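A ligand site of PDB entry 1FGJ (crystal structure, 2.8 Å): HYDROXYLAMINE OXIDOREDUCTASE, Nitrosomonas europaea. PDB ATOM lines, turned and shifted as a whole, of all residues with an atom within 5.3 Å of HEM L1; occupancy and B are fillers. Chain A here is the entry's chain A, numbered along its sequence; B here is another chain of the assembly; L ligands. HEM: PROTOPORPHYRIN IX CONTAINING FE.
Residues that only touch HEM L1: His 149, Ala 74, Glu 86, Cys 145, Ile 146, Pro 67, Met 166, Ile 164, Glu 72, Ala 158 and Asp 78.
Within 4 Å of HEM L1: Tyr 57, Tyr 64, Pro 67, Ser 69, Glu 72, Ala 74, Asp 78, Cys 79, Cys 82, His 83, Glu 86, Cys 145, Ile 146, His 149, Ala 158, His 160, Ile 164, Met 166, Ser 365 of chain B, Glu 366 of chain B and Arg 367 of chain B.
A carbon (CAC) of HEM L1 is bonded to the side-chain sulfur of Cys 82 (1.8 Å).
The side-chain sulfur (SG) of Cys 79 is bonded to a carbon (CAB) of HEM L1.
An iron atom (FE) of HEM L1 is bound by a ring nitrogen (NE2) of His 83 (2.1 Å).
An iron atom (FE) of HEM L1 is bound by a ring nitrogen (NE2) of His 160.
The side-chain hydroxyl of Tyr 64 is in hydrogen-bond range of an oxygen (O2A) of HEM L1 (2.7 Å).
O1A of HEM L1 is in hydrogen-bond range of OG of Ser 365 of chain B (2.7 Å).
The backbone NH of Arg 367 of chain B sits at hydrogen-bond distance from an oxygen (O2D) of HEM L1 (2.9 Å).
The guanidinium group of Arg 367 of chain B is in salt-bridge range of an oxygen (O2A) of HEM L1 (2.8 Å).
The side-chain hydroxyl (OH) of Tyr 57 sits at hydrogen-bond distance from an oxygen (O1A) of HEM L1.
An oxygen (O2D) of HEM L1 sits at hydrogen-bond distance from the backbone NH (N) of Glu 366 of chain B (3.1 Å).
An oxygen (O1D) of HEM L1 sits at hydrogen-bond distance from the side-chain hydroxyl (OG) of Ser 69 (3.5 Å).
N of Ser 365 of chain B sits at hydrogen-bond distance from O1A of HEM L2.
O of Tyr 57 lies close to O2D of HEM L2, at 2.8 Å.
An iron atom (FE) of HEM L2 is bound by a ring nitrogen (NE2) of His 149 (2.1 Å).
The side-chain sulfur (SG) of Cys 145 is covalently linked to a carbon (CAB) of HEM L2 (1.8 Å).
N of His 160 is in hydrogen-bond range of O of Glu 72 (2.7 Å).
The side-chain hydroxyl (OH) of Tyr 64 lies within hydrogen-bond range of the guanidinium group (NH1) of Arg 367 of chain B (3.1 Å).
OG of Ser 365 of chain B sits close to N of Phe 368 of chain B (3.3 Å).
The guanidinium group (NH2) of Arg 367 of chain B sits at hydrogen-bond distance from the backbone carbonyl oxygen (O) of Lys 65 (2.6 Å).
The side-chain hydroxyl of Tyr 57 sits at hydrogen-bond distance from the backbone NH of Phe 368 of chain B (3.4 Å).
ND1 of His 149 is in hydrogen-bond range of O of Arg 165.
The backbone carbonyl oxygen (O) of Ala 74 sits at hydrogen-bond distance from the backbone NH (N) of Ala 158.
OD2 of Asp 78 lies within hydrogen-bond range of N of Glu 75 (3.0 Å).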
ATOM      1  N   ILE A  56       0.367   3.047 -18.207  1.00  0.00           N
ATOM      2  CA  ILE A  56       0.202   3.320 -19.639  1.00  0.00           C
ATOM      3  C   ILE A  56      -0.771   4.483 -19.881  1.00  0.00           C
ATOM      4  O   ILE A  56      -0.809   5.059 -20.966  1.00  0.00           O
ATOM      5  CB  ILE A  56      -0.275   2.068 -20.421  1.00  0.00           C
ATOM      6  CG1 ILE A  56      -1.625   1.598 -19.894  1.00  0.00           C
ATOM      7  CG2 ILE A  56       0.743   0.955 -20.283  1.00  0.00           C
ATOM      8  CD1 ILE A  56      -2.211   0.448 -20.667  1.00  0.00           C
ATOM      9  N   TYR A  57      -1.542   4.816 -18.847  1.00  0.00           N
ATOM     10  CA  TYR A  57      -2.511   5.891 -18.871  1.00  0.00           C
ATOM     11  C   TYR A  57      -1.947   7.170 -18.262  1.00  0.00           C
ATOM     12  O   TYR A  57      -2.267   8.282 -18.692  1.00  0.00           O
ATOM     13  CB  TYR A  57      -3.764   5.454 -18.097  1.00  0.00           C
ATOM     14  CG  TYR A  57      -4.429   4.254 -18.716  1.00  0.00           C
ATOM     15  CD1 TYR A  57      -4.868   4.286 -20.036  1.00  0.00           C
ATOM     16  CD2 TYR A  57      -4.592   3.070 -17.999  1.00  0.00           C
ATOM     17  CE1 TYR A  57      -5.429   3.170 -20.637  1.00  0.00           C
ATOM     18  CE2 TYR A  57      -5.168   1.957 -18.583  1.00  0.00           C
ATOM     19  CZ  TYR A  57      -5.585   2.021 -19.912  1.00  0.00           C
ATOM     20  OH  TYR A  57      -6.160   0.924 -20.521  1.00  0.00           O
ATOM     21  N   TYR A  64       2.227   3.549 -23.166  1.00  0.00           N
ATOM     22  CA  TYR A  64       1.051   3.045 -23.867  1.00  0.00           C
ATOM     23  C   TYR A  64       1.259   2.296 -25.165  1.00  0.00           C
ATOM     24  O   TYR A  64       1.968   2.754 -26.064  1.00  0.00           O
ATOM     25  CB  TYR A  64      -0.020   4.125 -24.070  1.00  0.00           C
ATOM     26  CG  TYR A  64      -1.318   3.541 -24.567  1.00  0.00           C
ATOM     27  CD1 TYR A  64      -2.212   2.942 -23.684  1.00  0.00           C
ATOM     28  CD2 TYR A  64      -1.613   3.498 -25.936  1.00  0.00           C
ATOM     29  CE1 TYR A  64      -3.358   2.313 -24.150  1.00  0.00           C
ATOM     30  CE2 TYR A  64      -2.749   2.872 -26.411  1.00  0.00           C
ATOM     31  CZ  TYR A  64      -3.611   2.281 -25.513  1.00  0.00           C
ATOM     32  OH  TYR A  64      -4.740   1.652 -25.982  1.00  0.00           O
ATOM     33  N   LYS A  65       0.580   1.158 -25.267  1.00  0.00           N
ATOM     34  CA  LYS A  65       0.599   0.300 -26.439  1.00  0.00           C
ATOM     35  C   LYS A  65      -0.871  -0.110 -26.616  1.00  0.00           C
ATOM     36  O   LYS A  65      -1.581  -0.330 -25.628  1.00  0.00           O
ATOM     37  CB  LYS A  65       1.509  -0.913 -26.214  1.00  0.00           C
ATOM     38  CG  LYS A  65       0.974  -1.991 -25.281  1.00  0.00           C
ATOM     39  CD  LYS A  65       0.414  -3.189 -26.072  1.00  0.00           C
ATOM     40  CE  LYS A  65       0.028  -4.348 -25.152  1.00  0.00           C
ATOM     41  NZ  LYS A  65       1.210  -5.029 -24.528  1.00  0.00           N
ATOM     42  N   PRO A  67      -4.500  -1.937 -27.246  1.00  0.00           N
ATOM     43  CA  PRO A  67      -5.045  -3.174 -26.663  1.00  0.00           C
ATOM     44  C   PRO A  67      -5.227  -4.241 -27.741  1.00  0.00           C
ATOM     45  O   PRO A  67      -6.162  -4.180 -28.547  1.00  0.00           O
ATOM     46  CB  PRO A  67      -6.393  -2.714 -26.103  1.00  0.00           C
ATOM     47  CG  PRO A  67      -6.821  -1.688 -27.110  1.00  0.00           C
ATOM     48  CD  PRO A  67      -5.549  -0.908 -27.357  1.00  0.00           C
ATOM     49  N   SER A  69      -6.341  -7.059 -27.493  1.00  0.00           N
ATOM     50  CA  SER A  69      -7.501  -7.905 -27.211  1.00  0.00           C
ATOM     51  C   SER A  69      -8.432  -8.029 -28.423  1.00  0.00           C
ATOM     52  O   SER A  69      -8.693  -9.147 -28.888  1.00  0.00           O
ATOM     53  CB  SER A  69      -8.289  -7.401 -25.979  1.00  0.00           C
ATOM     54  OG  SER A  69      -7.453  -6.993 -24.909  1.00  0.00           O
ATOM     55  N   PRO A  70      -8.976  -6.912 -28.930  1.00  0.00           N
ATOM     56  CA  PRO A  70      -9.863  -7.027 -30.094  1.00  0.00           C
ATOM     57  C   PRO A  70      -9.154  -6.745 -31.421  1.00  0.00           C
ATOM     58  O   PRO A  70      -8.612  -5.654 -31.621  1.00  0.00           O
ATOM     59  CB  PRO A  70     -10.927  -5.978 -29.796  1.00  0.00           C
ATOM     60  CG  PRO A  70     -10.106  -4.868 -29.248  1.00  0.00           C
ATOM     61  CD  PRO A  70      -9.080  -5.548 -28.349  1.00  0.00           C
ATOM     62  N   GLU A  72      -9.597  -5.603 -34.596  1.00  0.00           N
ATOM     63  CA  GLU A  72     -10.544  -4.879 -35.421  1.00  0.00           C
ATOM     64  C   GLU A  72      -9.929  -3.745 -36.233  1.00  0.00           C
ATOM     65  O   GLU A  72      -9.049  -3.030 -35.749  1.00  0.00           O
ATOM     66  CB  GLU A  72     -11.674  -4.316 -34.561  1.00  0.00           C
ATOM     67  CG  GLU A  72     -12.757  -5.316 -34.200  1.00  0.00           C
ATOM     68  CD  GLU A  72     -13.617  -5.711 -35.407  1.00  0.00           C
ATOM     69  OE1 GLU A  72     -13.677  -4.939 -36.384  1.00  0.00           O
ATOM     70  OE2 GLU A  72     -14.242  -6.799 -35.345  1.00  0.00           O
ATOM     71  N   ALA A  74     -11.288  -0.553 -37.993  1.00  0.00           N
ATOM     72  CA  ALA A  74     -12.484   0.260 -38.039  1.00  0.00           C
ATOM     73  C   ALA A  74     -12.355   1.624 -38.688  1.00  0.00           C
ATOM     74  O   ALA A  74     -11.259   2.103 -38.967  1.00  0.00           O
ATOM     75  CB  ALA A  74     -13.021   0.430 -36.640  1.00  0.00           C
ATOM     76  N   GLU A  75     -13.499   2.242 -38.935  1.00  0.00           N
ATOM     77  CA  GLU A  75     -13.565   3.568 -39.527  1.00  0.00           C
ATOM     78  C   GLU A  75     -14.265   4.490 -38.529  1.00  0.00           C
ATOM     79  O   GLU A  75     -14.862   4.026 -37.555  1.00  0.00           O
ATOM     80  CB  GLU A  75     -14.380   3.530 -40.812  1.00  0.00           C
ATOM     81  CG  GLU A  75     -13.652   3.000 -42.022  1.00  0.00           C
ATOM     82  CD  GLU A  75     -14.465   3.186 -43.302  1.00  0.00           C
ATOM     83  OE1 GLU A  75     -14.700   4.366 -43.685  1.00  0.00           O
ATOM     84  OE2 GLU A  75     -14.892   2.177 -43.909  1.00  0.00           O
ATOM     85  N   ASP A  78     -17.526   3.391 -37.159  1.00  0.00           N
ATOM     86  CA  ASP A  78     -17.427   2.102 -36.448  1.00  0.00           C
ATOM     87  C   ASP A  78     -17.097   2.335 -34.988  1.00  0.00           C
ATOM     88  O   ASP A  78     -17.627   1.651 -34.103  1.00  0.00           O
ATOM     89  CB  ASP A  78     -16.300   1.240 -37.022  1.00  0.00           C
ATOM     90  CG  ASP A  78     -16.687   0.512 -38.269  1.00  0.00           C
ATOM     91  OD1 ASP A  78     -17.722  -0.183 -38.240  1.00  0.00           O
ATOM     92  OD2 ASP A  78     -15.944   0.606 -39.270  1.00  0.00           O
ATOM     93  N   CYS A  79     -16.176   3.277 -34.741  1.00  0.00           N
ATOM     94  CA  CYS A  79     -15.738   3.613 -33.398  1.00  0.00           C
ATOM     95  C   CYS A  79     -16.943   3.906 -32.528  1.00  0.00           C
ATOM     96  O   CYS A  79     -17.139   3.305 -31.477  1.00  0.00           O
ATOM     97  CB  CYS A  79     -14.807   4.827 -33.427  1.00  0.00           C
ATOM     98  SG  CYS A  79     -13.563   4.801 -34.773  1.00  0.00           S
ATOM     99  N   CYS A  82     -19.758   0.574 -32.376  1.00  0.00           N
ATOM    100  CA  CYS A  82     -19.304  -0.493 -31.490  1.00  0.00           C
ATOM    101  C   CYS A  82     -19.260  -0.012 -30.059  1.00  0.00           C
ATOM    102  O   CYS A  82     -19.728  -0.694 -29.149  1.00  0.00           O
ATOM    103  CB  CYS A  82     -17.922  -1.016 -31.885  1.00  0.00           C
ATOM    104  SG  CYS A  82     -17.475  -2.506 -30.931  1.00  0.00           S
ATOM    105  N   HIS A  83     -18.699   1.173 -29.856  1.00  0.00           N
ATOM    106  CA  HIS A  83     -18.605   1.696 -28.507  1.00  0.00           C
ATOM    107  C   HIS A  83     -19.926   2.087 -27.867  1.00  0.00           C
ATOM    108  O   HIS A  83     -19.985   2.215 -26.647  1.00  0.00           O
ATOM    109  CB  HIS A  83     -17.554   2.800 -28.421  1.00  0.00           C
ATOM    110  CG  HIS A  83     -16.164   2.270 -28.277  1.00  0.00           C
ATOM    111  ND1 HIS A  83     -15.644   1.806 -27.093  1.00  0.00           N
ATOM    112  CD2 HIS A  83     -15.204   2.075 -29.208  1.00  0.00           C
ATOM    113  CE1 HIS A  83     -14.415   1.335 -27.331  1.00  0.00           C
ATOM    114  NE2 HIS A  83     -14.101   1.480 -28.600  1.00  0.00           N
ATOM    115  N   GLU A  86     -20.115  -1.099 -26.233  1.00  0.00           N
ATOM    116  CA  GLU A  86     -18.918  -1.340 -25.434  1.00  0.00           C
ATOM    117  C   GLU A  86     -18.649  -0.352 -24.299  1.00  0.00           C
ATOM    118  O   GLU A  86     -18.297  -0.751 -23.199  1.00  0.00           O
ATOM    119  CB  GLU A  86     -17.666  -1.492 -26.308  1.00  0.00           C
ATOM    120  CG  GLU A  86     -17.554  -2.862 -26.977  1.00  0.00           C
ATOM    121  CD  GLU A  86     -17.469  -4.020 -25.980  1.00  0.00           C
ATOM    122  OE1 GLU A  86     -16.948  -3.832 -24.867  1.00  0.00           O
ATOM    123  OE2 GLU A  86     -17.931  -5.139 -26.321  1.00  0.00           O
ATOM    124  N   CYS A 145     -13.926  10.265 -31.920  1.00  0.00           N
ATOM    125  CA  CYS A 145     -13.013   9.286 -31.321  1.00  0.00           C
ATOM    126  C   CYS A 145     -11.762   9.032 -32.162  1.00  0.00           C
ATOM    127  O   CYS A 145     -10.654   9.134 -31.670  1.00  0.00           O
ATOM    128  CB  CYS A 145     -13.732   7.949 -31.053  1.00  0.00           C
ATOM    129  SG  CYS A 145     -15.548   7.971 -30.778  1.00  0.00           S
ATOM    130  N   ILE A 146     -11.933   8.742 -33.451  1.00  0.00           N
ATOM    131  CA  ILE A 146     -10.819   8.458 -34.372  1.00  0.00           C
ATOM    132  C   ILE A 146      -9.810   9.596 -34.518  1.00  0.00           C
ATOM    133  O   ILE A 146      -8.631   9.367 -34.811  1.00  0.00           O
ATOM    134  CB  ILE A 146     -11.372   8.076 -35.796  1.00  0.00           C
ATOM    135  CG1 ILE A 146     -10.316   7.328 -36.610  1.00  0.00           C
ATOM    136  CG2 ILE A 146     -11.843   9.317 -36.556  1.00  0.00           C
ATOM    137  CD1 ILE A 146     -10.858   6.754 -37.900  1.00  0.00           C
ATOM    138  N   HIS A 149      -7.999   9.519 -30.956  1.00  0.00           N
ATOM    139  CA  HIS A 149      -7.407   8.219 -30.703  1.00  0.00           C
ATOM    140  C   HIS A 149      -6.590   7.521 -31.775  1.00  0.00           C
ATOM    141  O   HIS A 149      -6.224   6.374 -31.610  1.00  0.00           O
ATOM    142  CB  HIS A 149      -8.443   7.279 -30.121  1.00  0.00           C
ATOM    143  CG  HIS A 149      -8.850   7.636 -28.718  1.00  0.00           C
ATOM    144  ND1 HIS A 149      -8.074   7.386 -27.610  1.00  0.00           N
ATOM    145  CD2 HIS A 149      -9.947   8.292 -28.267  1.00  0.00           C
ATOM    146  CE1 HIS A 149      -8.711   7.873 -26.547  1.00  0.00           C
ATOM    147  NE2 HIS A 149      -9.848   8.434 -26.888  1.00  0.00           N
ATOM    148  N   VAL A 150      -6.321   8.218 -32.878  1.00  0.00           N
ATOM    149  CA  VAL A 150      -5.511   7.672 -33.954  1.00  0.00           C
ATOM    150  C   VAL A 150      -4.858   8.828 -34.689  1.00  0.00           C
ATOM    151  O   VAL A 150      -3.673   9.101 -34.495  1.00  0.00           O
ATOM    152  CB  VAL A 150      -6.305   6.800 -34.980  1.00  0.00           C
ATOM    153  CG1 VAL A 150      -5.383   6.355 -36.086  1.00  0.00           C
ATOM    154  CG2 VAL A 150      -6.890   5.586 -34.327  1.00  0.00           C
ATOM    155  N   ALA A 158      -8.725   2.484 -39.426  1.00  0.00           N
ATOM    156  CA  ALA A 158      -7.668   2.421 -38.430  1.00  0.00           C
ATOM    157  C   ALA A 158      -7.658   0.995 -37.883  1.00  0.00           C
ATOM    158  O   ALA A 158      -8.704   0.362 -37.754  1.00  0.00           O
ATOM    159  CB  ALA A 158      -7.959   3.413 -37.306  1.00  0.00           C
ATOM    160  N   HIS A 160      -7.292  -1.206 -34.931  1.00  0.00           N
ATOM    161  CA  HIS A 160      -7.440  -1.101 -33.487  1.00  0.00           C
ATOM    162  C   HIS A 160      -6.209  -1.527 -32.685  1.00  0.00           C
ATOM    163  O   HIS A 160      -5.747  -0.773 -31.813  1.00  0.00           O
ATOM    164  CB  HIS A 160      -8.657  -1.917 -33.026  1.00  0.00           C
ATOM    165  CG  HIS A 160      -9.242  -1.448 -31.736  1.00  0.00           C
ATOM    166  ND1 HIS A 160      -8.864  -1.909 -30.491  1.00  0.00           N
ATOM    167  CD2 HIS A 160     -10.243  -0.551 -31.511  1.00  0.00           C
ATOM    168  CE1 HIS A 160      -9.633  -1.291 -29.580  1.00  0.00           C
ATOM    169  NE2 HIS A 160     -10.483  -0.459 -30.158  1.00  0.00           N
ATOM    170  N   ILE A 164      -4.427   2.552 -32.230  1.00  0.00           N
ATOM    171  CA  ILE A 164      -4.964   3.301 -31.099  1.00  0.00           C
ATOM    172  C   ILE A 164      -3.916   3.925 -30.163  1.00  0.00           C
ATOM    173  O   ILE A 164      -2.934   3.297 -29.776  1.00  0.00           O
ATOM    174  CB  ILE A 164      -5.940   2.429 -30.277  1.00  0.00           C
ATOM    175  CG1 ILE A 164      -7.200   2.160 -31.092  1.00  0.00           C
ATOM    176  CG2 ILE A 164      -6.300   3.093 -28.945  1.00  0.00           C
ATOM    177  CD1 ILE A 164      -7.917   3.418 -31.520  1.00  0.00           C
ATOM    178  N   ARG A 165      -4.162   5.175 -29.785  1.00  0.00           N
ATOM    179  CA  ARG A 165      -3.274   5.907 -28.890  1.00  0.00           C
ATOM    180  C   ARG A 165      -4.108   6.593 -27.820  1.00  0.00           C
ATOM    181  O   ARG A 165      -5.336   6.621 -27.898  1.00  0.00           O
ATOM    182  CB  ARG A 165      -2.504   6.999 -29.656  1.00  0.00           C
ATOM    183  CG  ARG A 165      -3.377   8.211 -29.968  1.00  0.00           C
ATOM    184  CD  ARG A 165      -2.678   9.277 -30.775  1.00  0.00           C
ATOM    185  NE  ARG A 165      -3.638  10.309 -31.179  1.00  0.00           N
ATOM    186  CZ  ARG A 165      -3.424  11.213 -32.133  1.00  0.00           C
ATOM    187  NH1 ARG A 165      -2.281  11.247 -32.795  1.00  0.00           N
ATOM    188  NH2 ARG A 165      -4.414  12.048 -32.468  1.00  0.00           N
ATOM    189  N   MET A 166      -3.428   7.129 -26.803  1.00  0.00           N
ATOM    190  CA  MET A 166      -4.063   7.877 -25.735  1.00  0.00           C
ATOM    191  C   MET A 166      -3.636   9.325 -25.963  1.00  0.00           C
ATOM    192  O   MET A 166      -2.445   9.626 -25.995  1.00  0.00           O
ATOM    193  CB  MET A 166      -3.569   7.400 -24.362  1.00  0.00           C
ATOM    194  CG  MET A 166      -4.131   6.074 -23.906  1.00  0.00           C
ATOM    195  SD  MET A 166      -5.920   6.052 -23.678  1.00  0.00           S
ATOM    196  CE  MET A 166      -6.356   4.586 -24.626  1.00  0.00           C
ATOM    197  N   SER B 365     -12.754   1.600 -20.188  1.00  0.00           N
ATOM    198  CA  SER B 365     -12.364   0.397 -20.914  1.00  0.00           C
ATOM    199  C   SER B 365     -12.029  -0.667 -19.868  1.00  0.00           C
ATOM    200  O   SER B 365     -11.589  -0.345 -18.779  1.00  0.00           O
ATOM    201  CB  SER B 365     -11.156   0.655 -21.808  1.00  0.00           C
ATOM    202  OG  SER B 365     -10.049   1.131 -21.061  1.00  0.00           O
ATOM    203  N   GLU B 366     -12.250  -1.934 -20.197  1.00  0.00           N
ATOM    204  CA  GLU B 366     -11.960  -2.994 -19.240  1.00  0.00           C
ATOM    205  C   GLU B 366     -10.500  -2.986 -18.845  1.00  0.00           C
ATOM    206  O   GLU B 366     -10.165  -3.180 -17.682  1.00  0.00           O
ATOM    207  CB  GLU B 366     -12.316  -4.363 -19.804  1.00  0.00           C
ATOM    208  CG  GLU B 366     -12.287  -5.423 -18.734  1.00  0.00           C
ATOM    209  CD  GLU B 366     -12.229  -6.806 -19.274  1.00  0.00           C
ATOM    210  OE1 GLU B 366     -11.324  -7.077 -20.088  1.00  0.00           O
ATOM    211  OE2 GLU B 366     -13.064  -7.640 -18.878  1.00  0.00           O
ATOM    212  N   ARG B 367      -9.640  -2.751 -19.819  1.00  0.00           N
ATOM    213  CA  ARG B 367      -8.206  -2.692 -19.604  1.00  0.00           C
ATOM    214  C   ARG B 367      -7.938  -1.649 -18.537  1.00  0.00           C
ATOM    215  O   ARG B 367      -7.191  -1.904 -17.597  1.00  0.00           O
ATOM    216  CB  ARG B 367      -7.529  -2.308 -20.914  1.00  0.00           C
ATOM    217  CG  ARG B 367      -6.021  -2.421 -20.944  1.00  0.00           C
ATOM    218  CD  ARG B 367      -5.494  -1.929 -22.275  1.00  0.00           C
ATOM    219  NE  ARG B 367      -4.050  -2.098 -22.430  1.00  0.00           N
ATOM    220  CZ  ARG B 367      -3.334  -1.526 -23.393  1.00  0.00           C
ATOM    221  NH1 ARG B 367      -3.913  -0.750 -24.287  1.00  0.00           N
ATOM    222  NH2 ARG B 367      -2.026  -1.750 -23.456  1.00  0.00           N
ATOM    223  N   PHE B 368      -8.594  -0.502 -18.650  1.00  0.00           N
ATOM    224  CA  PHE B 368      -8.451   0.592 -17.701  1.00  0.00           C
ATOM    225  C   PHE B 368      -9.005   0.220 -16.320  1.00  0.00           C
ATOM    226  O   PHE B 368      -8.355   0.464 -15.305  1.00  0.00           O
ATOM    227  CB  PHE B 368      -9.145   1.854 -18.229  1.00  0.00           C
ATOM    228  CG  PHE B 368      -9.109   3.031 -17.283  1.00  0.00           C
ATOM    229  CD1 PHE B 368     -10.127   3.229 -16.349  1.00  0.00           C
ATOM    230  CD2 PHE B 368      -8.070   3.956 -17.324  1.00  0.00           C
ATOM    231  CE1 PHE B 368     -10.108   4.328 -15.496  1.00  0.00           C
ATOM    232  CE2 PHE B 368      -8.050   5.055 -16.470  1.00  0.00           C
ATOM    233  CZ  PHE B 368      -9.072   5.237 -15.555  1.00  0.00           C
HETATM  234  CHA HEM L   1     -11.129  -0.065 -26.402  1.00  0.00           C
HETATM  235  CHB HEM L   1     -11.024   3.705 -29.407  1.00  0.00           C
HETATM  236  CHC HEM L   1     -13.281   1.067 -32.733  1.00  0.00           C
HETATM  237  CHD HEM L   1     -14.244  -2.228 -29.382  1.00  0.00           C
HETATM  238  C1A HEM L   1     -10.741   1.109 -27.012  1.00  0.00           C
HETATM  239  C2A HEM L   1      -9.965   2.149 -26.385  1.00  0.00           C
HETATM  240  C3A HEM L   1      -9.995   3.233 -27.167  1.00  0.00           C
HETATM  241  C4A HEM L   1     -10.793   2.861 -28.323  1.00  0.00           C
HETATM  242  CMA HEM L   1      -9.304   4.549 -26.894  1.00  0.00           C
HETATM  243  CAA HEM L   1      -9.216   2.091 -25.072  1.00  0.00           C
HETATM  244  CBA HEM L   1      -7.996   1.173 -25.158  1.00  0.00           C
HETATM  245  CGA HEM L   1      -7.328   0.949 -23.831  1.00  0.00           C
HETATM  246  O1A HEM L   1      -8.029   0.753 -22.826  1.00  0.00           O
HETATM  247  O2A HEM L   1      -6.089   0.965 -23.792  1.00  0.00           O
HETATM  248  C1B HEM L   1     -11.647   3.300 -30.566  1.00  0.00           C
HETATM  249  C2B HEM L   1     -11.671   4.103 -31.737  1.00  0.00           C
HETATM  250  C3B HEM L   1     -12.210   3.309 -32.712  1.00  0.00           C
HETATM  251  C4B HEM L   1     -12.558   2.043 -32.107  1.00  0.00           C
HETATM  252  CMB HEM L   1     -11.224   5.535 -31.885  1.00  0.00           C
HETATM  253  CAB HEM L   1     -12.277   3.618 -34.219  1.00  0.00           C
HETATM  254  CBB HEM L   1     -10.894   3.808 -34.856  1.00  0.00           C
HETATM  255  C1C HEM L   1     -13.713  -0.082 -32.141  1.00  0.00           C
HETATM  256  C2C HEM L   1     -14.560  -1.073 -32.765  1.00  0.00           C
HETATM  257  C3C HEM L   1     -14.909  -1.916 -31.746  1.00  0.00           C
HETATM  258  C4C HEM L   1     -14.252  -1.514 -30.563  1.00  0.00           C
HETATM  259  CMC HEM L   1     -14.974  -1.153 -34.237  1.00  0.00           C
HETATM  260  CAC HEM L   1     -15.933  -3.004 -31.715  1.00  0.00           C
HETATM  261  CBC HEM L   1     -16.058  -4.049 -32.800  1.00  0.00           C
HETATM  262  C1D HEM L   1     -13.503  -1.912 -28.251  1.00  0.00           C
HETATM  263  C2D HEM L   1     -13.378  -2.731 -27.072  1.00  0.00           C
HETATM  264  C3D HEM L   1     -12.488  -2.187 -26.262  1.00  0.00           C
HETATM  265  C4D HEM L   1     -12.035  -0.988 -26.932  1.00  0.00           C
HETATM  266  CMD HEM L   1     -14.017  -4.073 -26.847  1.00  0.00           C
HETATM  267  CAD HEM L   1     -11.996  -2.810 -24.965  1.00  0.00           C
HETATM  268  CBD HEM L   1     -10.505  -3.148 -24.952  1.00  0.00           C
HETATM  269  CGD HEM L   1     -10.000  -3.463 -23.551  1.00  0.00           C
HETATM  270  O1D HEM L   1      -9.156  -4.369 -23.411  1.00  0.00           O
HETATM  271  O2D HEM L   1     -10.439  -2.783 -22.601  1.00  0.00           O
HETATM  272  NA  HEM L   1     -11.253   1.549 -28.215  1.00  0.00           N
HETATM  273  NB  HEM L   1     -12.195   2.025 -30.791  1.00  0.00           N
HETATM  274  NC  HEM L   1     -13.515  -0.389 -30.789  1.00  0.00           N
HETATM  275  ND  HEM L   1     -12.664  -0.838 -28.165  1.00  0.00           N
HETATM  276 FE   HEM L   1     -12.406   0.543 -29.510  1.00  0.00          FE
HETATM  277  CHA HEM L   2      -9.344   7.874 -22.914  1.00  0.00           C
HETATM  278  CHB HEM L   2     -12.673   5.922 -25.879  1.00  0.00           C
HETATM  279  CHC HEM L   2     -13.397  10.199 -27.943  1.00  0.00           C
HETATM  280  CHD HEM L   2      -9.697  11.991 -25.461  1.00  0.00           C
HETATM  281  C1A HEM L   2     -10.250   6.954 -23.474  1.00  0.00           C
HETATM  282  C2A HEM L   2     -10.478   5.565 -23.052  1.00  0.00           C
HETATM  283  C3A HEM L   2     -11.497   5.094 -23.830  1.00  0.00           C
HETATM  284  C4A HEM L   2     -11.803   6.095 -24.811  1.00  0.00           C
HETATM  285  CMA HEM L   2     -12.304   3.824 -23.668  1.00  0.00           C
HETATM  286  CAA HEM L   2      -9.617   4.696 -22.120  1.00  0.00           C
HETATM  287  CBA HEM L   2      -9.394   5.122 -20.674  1.00  0.00           C
HETATM  288  CGA HEM L   2     -10.687   5.362 -19.932  1.00  0.00           C
HETATM  289  O1A HEM L   2     -11.557   4.475 -19.965  1.00  0.00           O
HETATM  290  O2A HEM L   2     -10.818   6.423 -19.300  1.00  0.00           O
HETATM  291  C1B HEM L   2     -13.184   6.938 -26.695  1.00  0.00           C
HETATM  292  C2B HEM L   2     -14.404   6.813 -27.520  1.00  0.00           C
HETATM  293  C3B HEM L   2     -14.614   8.041 -28.063  1.00  0.00           C
HETATM  294  C4B HEM L   2     -13.576   8.907 -27.546  1.00  0.00           C
HETATM  295  CMB HEM L   2     -15.323   5.605 -27.655  1.00  0.00           C
HETATM  296  CAB HEM L   2     -15.746   8.451 -29.026  1.00  0.00           C
HETATM  297  CBB HEM L   2     -17.161   8.335 -28.506  1.00  0.00           C
HETATM  298  C1C HEM L   2     -12.399  11.027 -27.523  1.00  0.00           C
HETATM  299  C2C HEM L   2     -12.120  12.317 -28.119  1.00  0.00           C
HETATM  300  C3C HEM L   2     -11.012  12.790 -27.466  1.00  0.00           C
HETATM  301  C4C HEM L   2     -10.672  11.820 -26.431  1.00  0.00           C
HETATM  302  CMC HEM L   2     -12.928  13.016 -29.213  1.00  0.00           C
HETATM  303  CAC HEM L   2     -10.216  14.045 -27.791  1.00  0.00           C
HETATM  304  CBC HEM L   2     -10.920  15.347 -27.450  1.00  0.00           C
HETATM  305  C1D HEM L   2      -9.316  11.073 -24.493  1.00  0.00           C
HETATM  306  C2D HEM L   2      -8.345  11.328 -23.421  1.00  0.00           C
HETATM  307  C3D HEM L   2      -8.197  10.139 -22.765  1.00  0.00           C
HETATM  308  C4D HEM L   2      -9.115   9.180 -23.359  1.00  0.00           C
HETATM  309  CMD HEM L   2      -7.761  12.704 -23.023  1.00  0.00           C
HETATM  310  CAD HEM L   2      -7.257   9.908 -21.594  1.00  0.00           C
HETATM  311  CBD HEM L   2      -5.964   9.166 -21.928  1.00  0.00           C
HETATM  312  CGD HEM L   2      -5.035   8.991 -20.721  1.00  0.00           C
HETATM  313  O1D HEM L   2      -5.534   8.754 -19.600  1.00  0.00           O
HETATM  314  O2D HEM L   2      -3.803   9.078 -20.919  1.00  0.00           O
HETATM  315  NA  HEM L   2     -11.087   7.276 -24.562  1.00  0.00           N
HETATM  316  NB  HEM L   2     -12.734   8.249 -26.655  1.00  0.00           N
HETATM  317  NC  HEM L   2     -11.480  10.717 -26.502  1.00  0.00           N
HETATM  318  ND  HEM L   2      -9.833   9.781 -24.408  1.00  0.00           N
HETATM  319 FE   HEM L   2     -11.294   9.021 -25.494  1.00  0.00          FE
